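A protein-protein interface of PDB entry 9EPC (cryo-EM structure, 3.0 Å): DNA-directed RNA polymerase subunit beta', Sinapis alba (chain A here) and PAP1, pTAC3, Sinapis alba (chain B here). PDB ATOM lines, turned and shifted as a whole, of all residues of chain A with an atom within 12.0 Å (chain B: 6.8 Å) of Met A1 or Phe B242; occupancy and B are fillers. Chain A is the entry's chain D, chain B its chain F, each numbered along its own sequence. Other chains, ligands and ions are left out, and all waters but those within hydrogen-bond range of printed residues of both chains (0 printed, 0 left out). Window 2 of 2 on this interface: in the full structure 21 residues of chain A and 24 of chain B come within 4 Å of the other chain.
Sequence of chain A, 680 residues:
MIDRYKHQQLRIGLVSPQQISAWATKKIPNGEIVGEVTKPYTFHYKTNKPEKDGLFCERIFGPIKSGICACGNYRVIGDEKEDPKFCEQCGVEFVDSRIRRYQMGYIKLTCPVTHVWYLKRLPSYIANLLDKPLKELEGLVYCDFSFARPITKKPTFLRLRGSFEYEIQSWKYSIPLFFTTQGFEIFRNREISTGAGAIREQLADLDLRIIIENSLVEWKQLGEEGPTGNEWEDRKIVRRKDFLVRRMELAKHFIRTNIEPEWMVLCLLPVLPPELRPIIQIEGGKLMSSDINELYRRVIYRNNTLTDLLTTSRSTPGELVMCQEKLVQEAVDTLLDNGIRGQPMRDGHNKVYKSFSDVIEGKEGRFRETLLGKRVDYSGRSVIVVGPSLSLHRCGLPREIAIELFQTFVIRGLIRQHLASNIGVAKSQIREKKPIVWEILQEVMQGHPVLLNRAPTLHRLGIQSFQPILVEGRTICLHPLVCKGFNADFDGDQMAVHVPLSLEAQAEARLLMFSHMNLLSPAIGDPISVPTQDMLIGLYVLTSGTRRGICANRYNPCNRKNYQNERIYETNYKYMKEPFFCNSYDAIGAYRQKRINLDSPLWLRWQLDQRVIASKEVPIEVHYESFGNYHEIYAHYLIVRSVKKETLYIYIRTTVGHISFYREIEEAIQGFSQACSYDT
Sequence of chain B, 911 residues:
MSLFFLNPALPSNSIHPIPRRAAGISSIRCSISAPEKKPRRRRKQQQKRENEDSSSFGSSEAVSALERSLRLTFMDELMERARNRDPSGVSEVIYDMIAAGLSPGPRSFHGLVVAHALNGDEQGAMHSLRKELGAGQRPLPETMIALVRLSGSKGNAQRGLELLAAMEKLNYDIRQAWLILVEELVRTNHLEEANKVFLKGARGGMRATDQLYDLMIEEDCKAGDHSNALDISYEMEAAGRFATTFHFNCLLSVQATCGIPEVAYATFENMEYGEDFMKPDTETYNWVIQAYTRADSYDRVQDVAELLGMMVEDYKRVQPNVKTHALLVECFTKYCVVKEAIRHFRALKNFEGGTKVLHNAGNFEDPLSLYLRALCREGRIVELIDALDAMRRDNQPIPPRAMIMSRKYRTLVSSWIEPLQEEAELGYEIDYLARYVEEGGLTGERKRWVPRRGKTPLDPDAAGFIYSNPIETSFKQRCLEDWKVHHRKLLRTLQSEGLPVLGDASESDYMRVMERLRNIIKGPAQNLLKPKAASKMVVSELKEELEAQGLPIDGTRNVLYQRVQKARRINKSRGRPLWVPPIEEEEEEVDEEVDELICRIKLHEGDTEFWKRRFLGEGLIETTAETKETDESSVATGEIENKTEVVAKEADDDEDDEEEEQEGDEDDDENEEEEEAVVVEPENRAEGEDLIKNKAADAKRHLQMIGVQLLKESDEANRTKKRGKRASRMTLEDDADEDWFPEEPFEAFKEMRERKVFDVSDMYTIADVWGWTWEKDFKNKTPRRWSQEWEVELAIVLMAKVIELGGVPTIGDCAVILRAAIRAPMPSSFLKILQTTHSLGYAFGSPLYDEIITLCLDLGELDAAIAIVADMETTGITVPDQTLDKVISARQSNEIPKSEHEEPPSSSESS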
ATOM      1  N   MET A   1      12.419 -14.292  28.744  1.00  0.00           N
ATOM      2  CA  MET A   1      12.814 -15.510  29.441  1.00  0.00           C
ATOM      3  C   MET A   1      13.312 -16.569  28.463  1.00  0.00           C
ATOM      4  O   MET A   1      12.569 -17.025  27.595  1.00  0.00           O
ATOM      5  CB  MET A   1      11.647 -16.067  30.249  1.00  0.00           C
ATOM      6  CG  MET A   1      12.052 -17.199  31.159  1.00  0.00           C
ATOM      7  SD  MET A   1      13.361 -16.675  32.277  1.00  0.00           S
ATOM      8  CE  MET A   1      12.492 -15.446  33.251  1.00  0.00           C
ATOM      9  N   ILE A   2      14.571 -16.972  28.617  1.00  0.00           N
ATOM     10  CA  ILE A   2      15.197 -17.902  27.685  1.00  0.00           C
ATOM     11  C   ILE A   2      14.794 -19.321  28.064  1.00  0.00           C
ATOM     12  O   ILE A   2      15.111 -19.799  29.155  1.00  0.00           O
ATOM     13  CB  ILE A   2      16.720 -17.747  27.673  1.00  0.00           C
ATOM     14  CG1 ILE A   2      17.093 -16.270  27.590  1.00  0.00           C
ATOM     15  CG2 ILE A   2      17.312 -18.496  26.494  1.00  0.00           C
ATOM     16  CD1 ILE A   2      18.564 -16.022  27.701  1.00  0.00           C
ATOM     17  N   ASP A   3      14.096 -19.996  27.157  1.00  0.00           N
ATOM     18  CA  ASP A   3      13.740 -21.389  27.363  1.00  0.00           C
ATOM     19  C   ASP A   3      14.984 -22.266  27.347  1.00  0.00           C
ATOM     20  O   ASP A   3      15.906 -22.053  26.556  1.00  0.00           O
ATOM     21  CB  ASP A   3      12.763 -21.850  26.283  1.00  0.00           C
ATOM     22  CG  ASP A   3      11.449 -21.103  26.333  1.00  0.00           C
ATOM     23  OD1 ASP A   3      11.297 -20.237  27.218  1.00  0.00           O
ATOM     24  OD2 ASP A   3      10.569 -21.377  25.490  1.00  0.00           O
ATOM     25  N   ARG A   4      15.003 -23.264  28.225  1.00  0.00           N
ATOM     26  CA  ARG A   4      16.108 -24.217  28.274  1.00  0.00           C
ATOM     27  C   ARG A   4      16.014 -25.106  27.043  1.00  0.00           C
ATOM     28  O   ARG A   4      15.327 -26.129  27.049  1.00  0.00           O
ATOM     29  CB  ARG A   4      16.048 -25.039  29.555  1.00  0.00           C
ATOM     30  CG  ARG A   4      16.043 -24.210  30.825  1.00  0.00           C
ATOM     31  CD  ARG A   4      17.347 -23.458  30.988  1.00  0.00           C
ATOM     32  NE  ARG A   4      18.492 -24.360  30.986  1.00  0.00           N
ATOM     33  CZ  ARG A   4      19.744 -23.980  31.205  1.00  0.00           C
ATOM     34  NH1 ARG A   4      20.048 -22.717  31.455  1.00  0.00           N
ATOM     35  NH2 ARG A   4      20.713 -24.890  31.174  1.00  0.00           N
ATOM     36  N   TYR A   5      16.707 -24.713  25.979  1.00  0.00           N
ATOM     37  CA  TYR A   5      16.564 -25.391  24.699  1.00  0.00           C
ATOM     38  C   TYR A   5      17.106 -26.811  24.781  1.00  0.00           C
ATOM     39  O   TYR A   5      18.185 -27.048  25.331  1.00  0.00           O
ATOM     40  CB  TYR A   5      17.289 -24.612  23.605  1.00  0.00           C
ATOM     41  CG  TYR A   5      16.880 -23.160  23.523  1.00  0.00           C
ATOM     42  CD1 TYR A   5      15.611 -22.800  23.097  1.00  0.00           C
ATOM     43  CD2 TYR A   5      17.766 -22.151  23.865  1.00  0.00           C
ATOM     44  CE1 TYR A   5      15.235 -21.475  23.019  1.00  0.00           C
ATOM     45  CE2 TYR A   5      17.401 -20.824  23.789  1.00  0.00           C
ATOM     46  CZ  TYR A   5      16.134 -20.491  23.366  1.00  0.00           C
ATOM     47  OH  TYR A   5      15.766 -19.169  23.290  1.00  0.00           O
ATOM     48  N   LYS A   6      16.347 -27.758  24.232  1.00  0.00           N
ATOM     49  CA  LYS A   6      16.755 -29.161  24.164  1.00  0.00           C
ATOM     50  C   LYS A   6      16.268 -29.699  22.822  1.00  0.00           C
ATOM     51  O   LYS A   6      15.122 -30.136  22.696  1.00  0.00           O
ATOM     52  CB  LYS A   6      16.199 -29.964  25.332  1.00  0.00           C
ATOM     53  CG  LYS A   6      16.622 -31.424  25.332  1.00  0.00           C
ATOM     54  CD  LYS A   6      16.009 -32.176  26.499  1.00  0.00           C
ATOM     55  CE  LYS A   6      14.492 -32.178  26.415  1.00  0.00           C
ATOM     56  NZ  LYS A   6      13.874 -32.893  27.566  1.00  0.00           N
ATOM     57  N   TYR B 234      22.046 -16.781  30.285  1.00  0.00           N
ATOM     58  CA  TYR B 234      21.376 -17.498  31.367  1.00  0.00           C
ATOM     59  C   TYR B 234      21.738 -16.908  32.723  1.00  0.00           C
ATOM     60  O   TYR B 234      20.878 -16.778  33.601  1.00  0.00           O
ATOM     61  CB  TYR B 234      21.733 -18.981  31.315  1.00  0.00           C
ATOM     62  CG  TYR B 234      20.977 -19.753  30.261  1.00  0.00           C
ATOM     63  CD1 TYR B 234      19.620 -19.552  30.068  1.00  0.00           C
ATOM     64  CD2 TYR B 234      21.623 -20.678  29.455  1.00  0.00           C
ATOM     65  CE1 TYR B 234      18.926 -20.253  29.107  1.00  0.00           C
ATOM     66  CE2 TYR B 234      20.936 -21.385  28.491  1.00  0.00           C
ATOM     67  CZ  TYR B 234      19.588 -21.167  28.320  1.00  0.00           C
ATOM     68  OH  TYR B 234      18.899 -21.868  27.359  1.00  0.00           O
ATOM     69  N   MET B 236      22.564 -13.822  33.273  1.00  0.00           N
ATOM     70  CA  MET B 236      21.837 -12.561  33.355  1.00  0.00           C
ATOM     71  C   MET B 236      20.394 -12.784  33.788  1.00  0.00           C
ATOM     72  O   MET B 236      19.862 -12.032  34.613  1.00  0.00           O
ATOM     73  CB  MET B 236      21.892 -11.844  32.009  1.00  0.00           C
ATOM     74  CG  MET B 236      20.939 -10.672  31.881  1.00  0.00           C
ATOM     75  SD  MET B 236      21.039  -9.921  30.248  1.00  0.00           S
ATOM     76  CE  MET B 236      20.742 -11.352  29.217  1.00  0.00           C
ATOM     77  N   GLU B 237      19.747 -13.817  33.243  1.00  0.00           N
ATOM     78  CA  GLU B 237      18.376 -14.125  33.636  1.00  0.00           C
ATOM     79  C   GLU B 237      18.293 -14.450  35.121  1.00  0.00           C
ATOM     80  O   GLU B 237      17.387 -13.986  35.821  1.00  0.00           O
ATOM     81  CB  GLU B 237      17.840 -15.288  32.800  1.00  0.00           C
ATOM     82  CG  GLU B 237      17.713 -14.991  31.317  1.00  0.00           C
ATOM     83  CD  GLU B 237      16.503 -14.139  30.991  1.00  0.00           C
ATOM     84  OE1 GLU B 237      15.737 -13.802  31.918  1.00  0.00           O
ATOM     85  OE2 GLU B 237      16.313 -13.808  29.803  1.00  0.00           O
ATOM     86  N   GLY B 240      18.439 -11.345  37.591  1.00  0.00           N
ATOM     87  CA  GLY B 240      17.323 -10.437  37.737  1.00  0.00           C
ATOM     88  C   GLY B 240      17.036  -9.562  36.539  1.00  0.00           C
ATOM     89  O   GLY B 240      16.113  -8.741  36.602  1.00  0.00           O
ATOM     90  N   ARG B 241      17.791  -9.702  35.454  1.00  0.00           N
ATOM     91  CA  ARG B 241      17.544  -8.968  34.222  1.00  0.00           C
ATOM     92  C   ARG B 241      17.122  -9.948  33.138  1.00  0.00           C
ATOM     93  O   ARG B 241      17.736 -11.008  32.981  1.00  0.00           O
ATOM     94  CB  ARG B 241      18.784  -8.194  33.775  1.00  0.00           C
ATOM     95  CG  ARG B 241      18.539  -7.323  32.559  1.00  0.00           C
ATOM     96  CD  ARG B 241      19.833  -6.847  31.932  1.00  0.00           C
ATOM     97  NE  ARG B 241      19.579  -5.997  30.776  1.00  0.00           N
ATOM     98  CZ  ARG B 241      20.514  -5.566  29.943  1.00  0.00           C
ATOM     99  NH1 ARG B 241      21.784  -5.898  30.096  1.00  0.00           N
ATOM    100  NH2 ARG B 241      20.164  -4.784  28.925  1.00  0.00           N
ATOM    101  N   PHE B 242      16.080  -9.596  32.396  1.00  0.00           N
ATOM    102  CA  PHE B 242      15.539 -10.464  31.364  1.00  0.00           C
ATOM    103  C   PHE B 242      16.050 -10.041  29.994  1.00  0.00           C
ATOM    104  O   PHE B 242      16.193  -8.852  29.702  1.00  0.00           O
ATOM    105  CB  PHE B 242      14.011 -10.443  31.384  1.00  0.00           C
ATOM    106  CG  PHE B 242      13.427 -10.615  32.752  1.00  0.00           C
ATOM    107  CD1 PHE B 242      13.577 -11.808  33.436  1.00  0.00           C
ATOM    108  CD2 PHE B 242      12.730  -9.584  33.357  1.00  0.00           C
ATOM    109  CE1 PHE B 242      13.043 -11.970  34.699  1.00  0.00           C
ATOM    110  CE2 PHE B 242      12.193  -9.740  34.618  1.00  0.00           C
ATOM    111  CZ  PHE B 242      12.350 -10.934  35.290  1.00  0.00           C
ATOM    112  N   ALA B 243      16.327 -11.034  29.155  1.00  0.00           N
ATOM    113  CA  ALA B 243      16.863 -10.774  27.826  1.00  0.00           C
ATOM    114  C   ALA B 243      15.800 -10.119  26.955  1.00  0.00           C
ATOM    115  O   ALA B 243      14.756 -10.719  26.682  1.00  0.00           O
ATOM    116  CB  ALA B 243      17.353 -12.071  27.190  1.00  0.00           C
ATOM    117  N   THR B 244      16.064  -8.892  26.521  1.00  0.00           N
ATOM    118  CA  THR B 244      15.147  -8.175  25.646  1.00  0.00           C
ATOM    119  C   THR B 244      15.357  -8.642  24.207  1.00  0.00           C
ATOM    120  O   THR B 244      16.038  -9.636  23.942  1.00  0.00           O
ATOM    121  CB  THR B 244      15.338  -6.669  25.793  1.00  0.00           C
ATOM    122  OG1 THR B 244      14.449  -5.985  24.902  1.00  0.00           O
ATOM    123  CG2 THR B 244      16.767  -6.279  25.464  1.00  0.00           C
ATOM    124  N   THR B 245      14.761  -7.925  23.252  1.00  0.00           N
ATOM    125  CA  THR B 245      14.923  -8.286  21.848  1.00  0.00           C
ATOM    126  C   THR B 245      16.376  -8.175  21.408  1.00  0.00           C
ATOM    127  O   THR B 245      16.831  -8.957  20.566  1.00  0.00           O
ATOM    128  CB  THR B 245      14.038  -7.402  20.970  1.00  0.00           C
ATOM    129  OG1 THR B 245      12.706  -7.384  21.498  1.00  0.00           O
ATOM    130  CG2 THR B 245      13.999  -7.934  19.548  1.00  0.00           C
ATOM    131  N   HIS B 247      19.175  -8.854  23.042  1.00  0.00           N
ATOM    132  CA  HIS B 247      19.987 -10.008  23.410  1.00  0.00           C
ATOM    133  C   HIS B 247      19.672 -11.213  22.536  1.00  0.00           C
ATOM    134  O   HIS B 247      20.580 -11.954  22.143  1.00  0.00           O
ATOM    135  CB  HIS B 247      19.780 -10.341  24.884  1.00  0.00           C
ATOM    136  CG  HIS B 247      20.200  -9.245  25.807  1.00  0.00           C
ATOM    137  ND1 HIS B 247      19.516  -8.053  25.906  1.00  0.00           N
ATOM    138  CD2 HIS B 247      21.246  -9.149  26.661  1.00  0.00           C
ATOM    139  CE1 HIS B 247      20.115  -7.276  26.789  1.00  0.00           C
ATOM    140  NE2 HIS B 247      21.168  -7.918  27.262  1.00  0.00           N
ATOM    141  N   PHE B 248      18.396 -11.428  22.223  1.00  0.00           N
ATOM    142  CA  PHE B 248      18.037 -12.544  21.355  1.00  0.00           C
ATOM    143  C   PHE B 248      18.559 -12.331  19.940  1.00  0.00           C
ATOM    144  O   PHE B 248      18.934 -13.293  19.261  1.00  0.00           O
ATOM    145  CB  PHE B 248      16.524 -12.743  21.350  1.00  0.00           C
ATOM    146  CG  PHE B 248      15.992 -13.371  22.602  1.00  0.00           C
ATOM    147  CD1 PHE B 248      16.206 -14.712  22.861  1.00  0.00           C
ATOM    148  CD2 PHE B 248      15.268 -12.624  23.515  1.00  0.00           C
ATOM    149  CE1 PHE B 248      15.716 -15.293  24.010  1.00  0.00           C
ATOM    150  CE2 PHE B 248      14.775 -13.204  24.665  1.00  0.00           C
ATOM    151  CZ  PHE B 248      14.999 -14.538  24.912  1.00  0.00           C
ATOM    152  N   ASN B 270      10.586 -18.706  21.371  1.00  0.00           N
ATOM    153  CA  ASN B 270      10.725 -18.277  22.757  1.00  0.00           C
ATOM    154  C   ASN B 270      10.511 -16.778  22.907  1.00  0.00           C
ATOM    155  O   ASN B 270      10.064 -16.319  23.963  1.00  0.00           O
ATOM    156  CB  ASN B 270      12.098 -18.678  23.293  1.00  0.00           C
ATOM    157  CG  ASN B 270      12.428 -18.010  24.609  1.00  0.00           C
ATOM    158  OD1 ASN B 270      13.466 -17.369  24.747  1.00  0.00           O
ATOM    159  ND2 ASN B 270      11.537 -18.146  25.583  1.00  0.00           N
ATOM    160  N   MET B 271      10.808 -16.001  21.867  1.00  0.00           N
ATOM    161  CA  MET B 271      10.611 -14.561  21.926  1.00  0.00           C
ATOM    162  C   MET B 271       9.366 -14.092  21.187  1.00  0.00           C
ATOM    163  O   MET B 271       8.841 -13.023  21.515  1.00  0.00           O
ATOM    164  CB  MET B 271      11.840 -13.832  21.368  1.00  0.00           C
ATOM    165  CG  MET B 271      12.094 -14.059  19.892  1.00  0.00           C
ATOM    166  SD  MET B 271      13.652 -13.336  19.353  1.00  0.00           S
ATOM    167  CE  MET B 271      13.347 -11.602  19.668  1.00  0.00           C
ATOM    168  N   GLY B 274       6.200 -14.319  23.794  1.00  0.00           N
ATOM    169  CA  GLY B 274       6.755 -13.880  25.057  1.00  0.00           C
ATOM    170  C   GLY B 274       6.274 -12.506  25.473  1.00  0.00           C
ATOM    171  O   GLY B 274       5.211 -12.055  25.038  1.00  0.00           O
ATOM    172  N   GLU B 275       7.050 -11.831  26.315  1.00  0.00           N
ATOM    173  CA  GLU B 275       6.669 -10.512  26.789  1.00  0.00           C
ATOM    174  C   GLU B 275       6.853  -9.471  25.688  1.00  0.00           C
ATOM    175  O   GLU B 275       7.369  -9.750  24.603  1.00  0.00           O
ATOM    176  CB  GLU B 275       7.479 -10.133  28.027  1.00  0.00           C
ATOM    177  CG  GLU B 275       6.875 -10.613  29.338  1.00  0.00           C
ATOM    178  CD  GLU B 275       6.764 -12.123  29.419  1.00  0.00           C
ATOM    179  OE1 GLU B 275       7.583 -12.818  28.784  1.00  0.00           O
ATOM    180  OE2 GLU B 275       5.853 -12.614  30.118  1.00  0.00           O
ATOM    181  N   PHE B 277       8.783  -6.731  25.612  1.00  0.00           N
ATOM    182  CA  PHE B 277      10.165  -6.374  25.323  1.00  0.00           C
ATOM    183  C   PHE B 277      10.914  -7.494  24.615  1.00  0.00           C
ATOM    184  O   PHE B 277      11.984  -7.248  24.050  1.00  0.00           O
ATOM    185  CB  PHE B 277      10.895  -5.983  26.608  1.00  0.00           C
ATOM    186  CG  PHE B 277      10.868  -7.040  27.672  1.00  0.00           C
ATOM    187  CD1 PHE B 277      11.861  -8.000  27.740  1.00  0.00           C
ATOM    188  CD2 PHE B 277       9.856  -7.066  28.615  1.00  0.00           C
ATOM    189  CE1 PHE B 277      11.840  -8.970  28.720  1.00  0.00           C
ATOM    190  CE2 PHE B 277       9.831  -8.034  29.598  1.00  0.00           C
ATOM    191  CZ  PHE B 277      10.825  -8.987  29.650  1.00  0.00           C
ATOM    192  N   MET B 278      10.381  -8.710  24.635  1.00  0.00           N
ATOM    193  CA  MET B 278      10.962  -9.830  23.913  1.00  0.00           C
ATOM    194  C   MET B 278      10.364 -10.011  22.526  1.00  0.00           C
ATOM    195  O   MET B 278      10.759 -10.939  21.815  1.00  0.00           O
ATOM    196  CB  MET B 278      10.787 -11.120  24.716  1.00  0.00           C
ATOM    197  CG  MET B 278      11.612 -11.182  25.985  1.00  0.00           C
ATOM    198  SD  MET B 278      11.069 -12.507  27.073  1.00  0.00           S
ATOM    199  CE  MET B 278      10.593 -13.743  25.872  1.00  0.00           C
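OD1 of Asp A3 is in hydrogen-bond range of ND2 of Asn B270 (2.7 Å). The backbone carbonyl oxygen of Asp A3 lies within hydrogen-bond range of the side-chain hydroxyl of Tyr B234, at 3.1 Å. The side-chain amide oxygen of Asn B270 lies within hydrogen-bond range of the side-chain hydroxyl of Tyr A5. O of Met A1 is in hydrogen-bond range of ND2 of Asn B270, 2.5 Å away. SD of Met A1 lies close to OE1 of Glu B237, 3.7 Å away. The backbone NH of Met A1 is in hydrogen-bond range of the side-chain sulfur of Met B278 (2.8 Å).
The backbone NH (N) of Ala B243 lies within hydrogen-bond range of the side-chain carboxylate (OE2) of Glu B237 (2.8 Å).
Among the printed residues, pairs that only touch across the chains: Arg A4 with Tyr B234, Ile A2 with Glu B237, Ile A2 with Asn B270, Ile A2 with Tyr B234, Tyr A5 with Tyr B234, Met A1 with Phe B242, Ile A2 with Phe B248 and Tyr A5 with Phe B248.
Of chain B, only Glu B237, Phe B242, Asn B270 and Met B278 come within 4 Å of Met A1. Printed residues of chain B within 4 Å of Asp A3: Tyr B234 (3.1 Å) and Asn B270 (2.7 Å). Printed residues of chain B within 4 Å of Tyr A5: Tyr B234 (3.7 Å), Phe B248 (3.9 Å) and Asn B270 (3.3 Å). No residue of chain A comes within 4 Å of Met B236. Glu B237 touches just these residues of chain A: Met A1 and Ile A2. No residue of chain A comes within 4 Å of Gly B240. No residue of chain A comes within 4 Å of Arg B241. No residue of chain A comes within 4 Å of Thr B244. Printed residues of chain A within 4 Å of Phe B248: Ile A2 (3.8 Å) and Tyr A5 (3.9 Å). Of chain A, only Met A1 (2.5 Å), Ile A2 (3.5 Å), Asp A3 (2.7 Å) and Tyr A5 (3.3 Å) come within 4 Å of Asn B270. Gly B274 touches none of the printed residues of chain A. Met B278 touches just one residue of chain A: Met A1 (2.8 Å). The nearest printed residue of chain B that does not touch Ile A2 is Ala B243 (4.2 Å).
Of the 6 printed residues of chain A, 5 touch a printed residue of chain B. Hydrophobic or aromatic side chains of chain A within 4 Å of the printed part of chain B: Met A1, Ile A2 and Tyr A5. Among the printed residues, 14 pairs touch across the chains.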
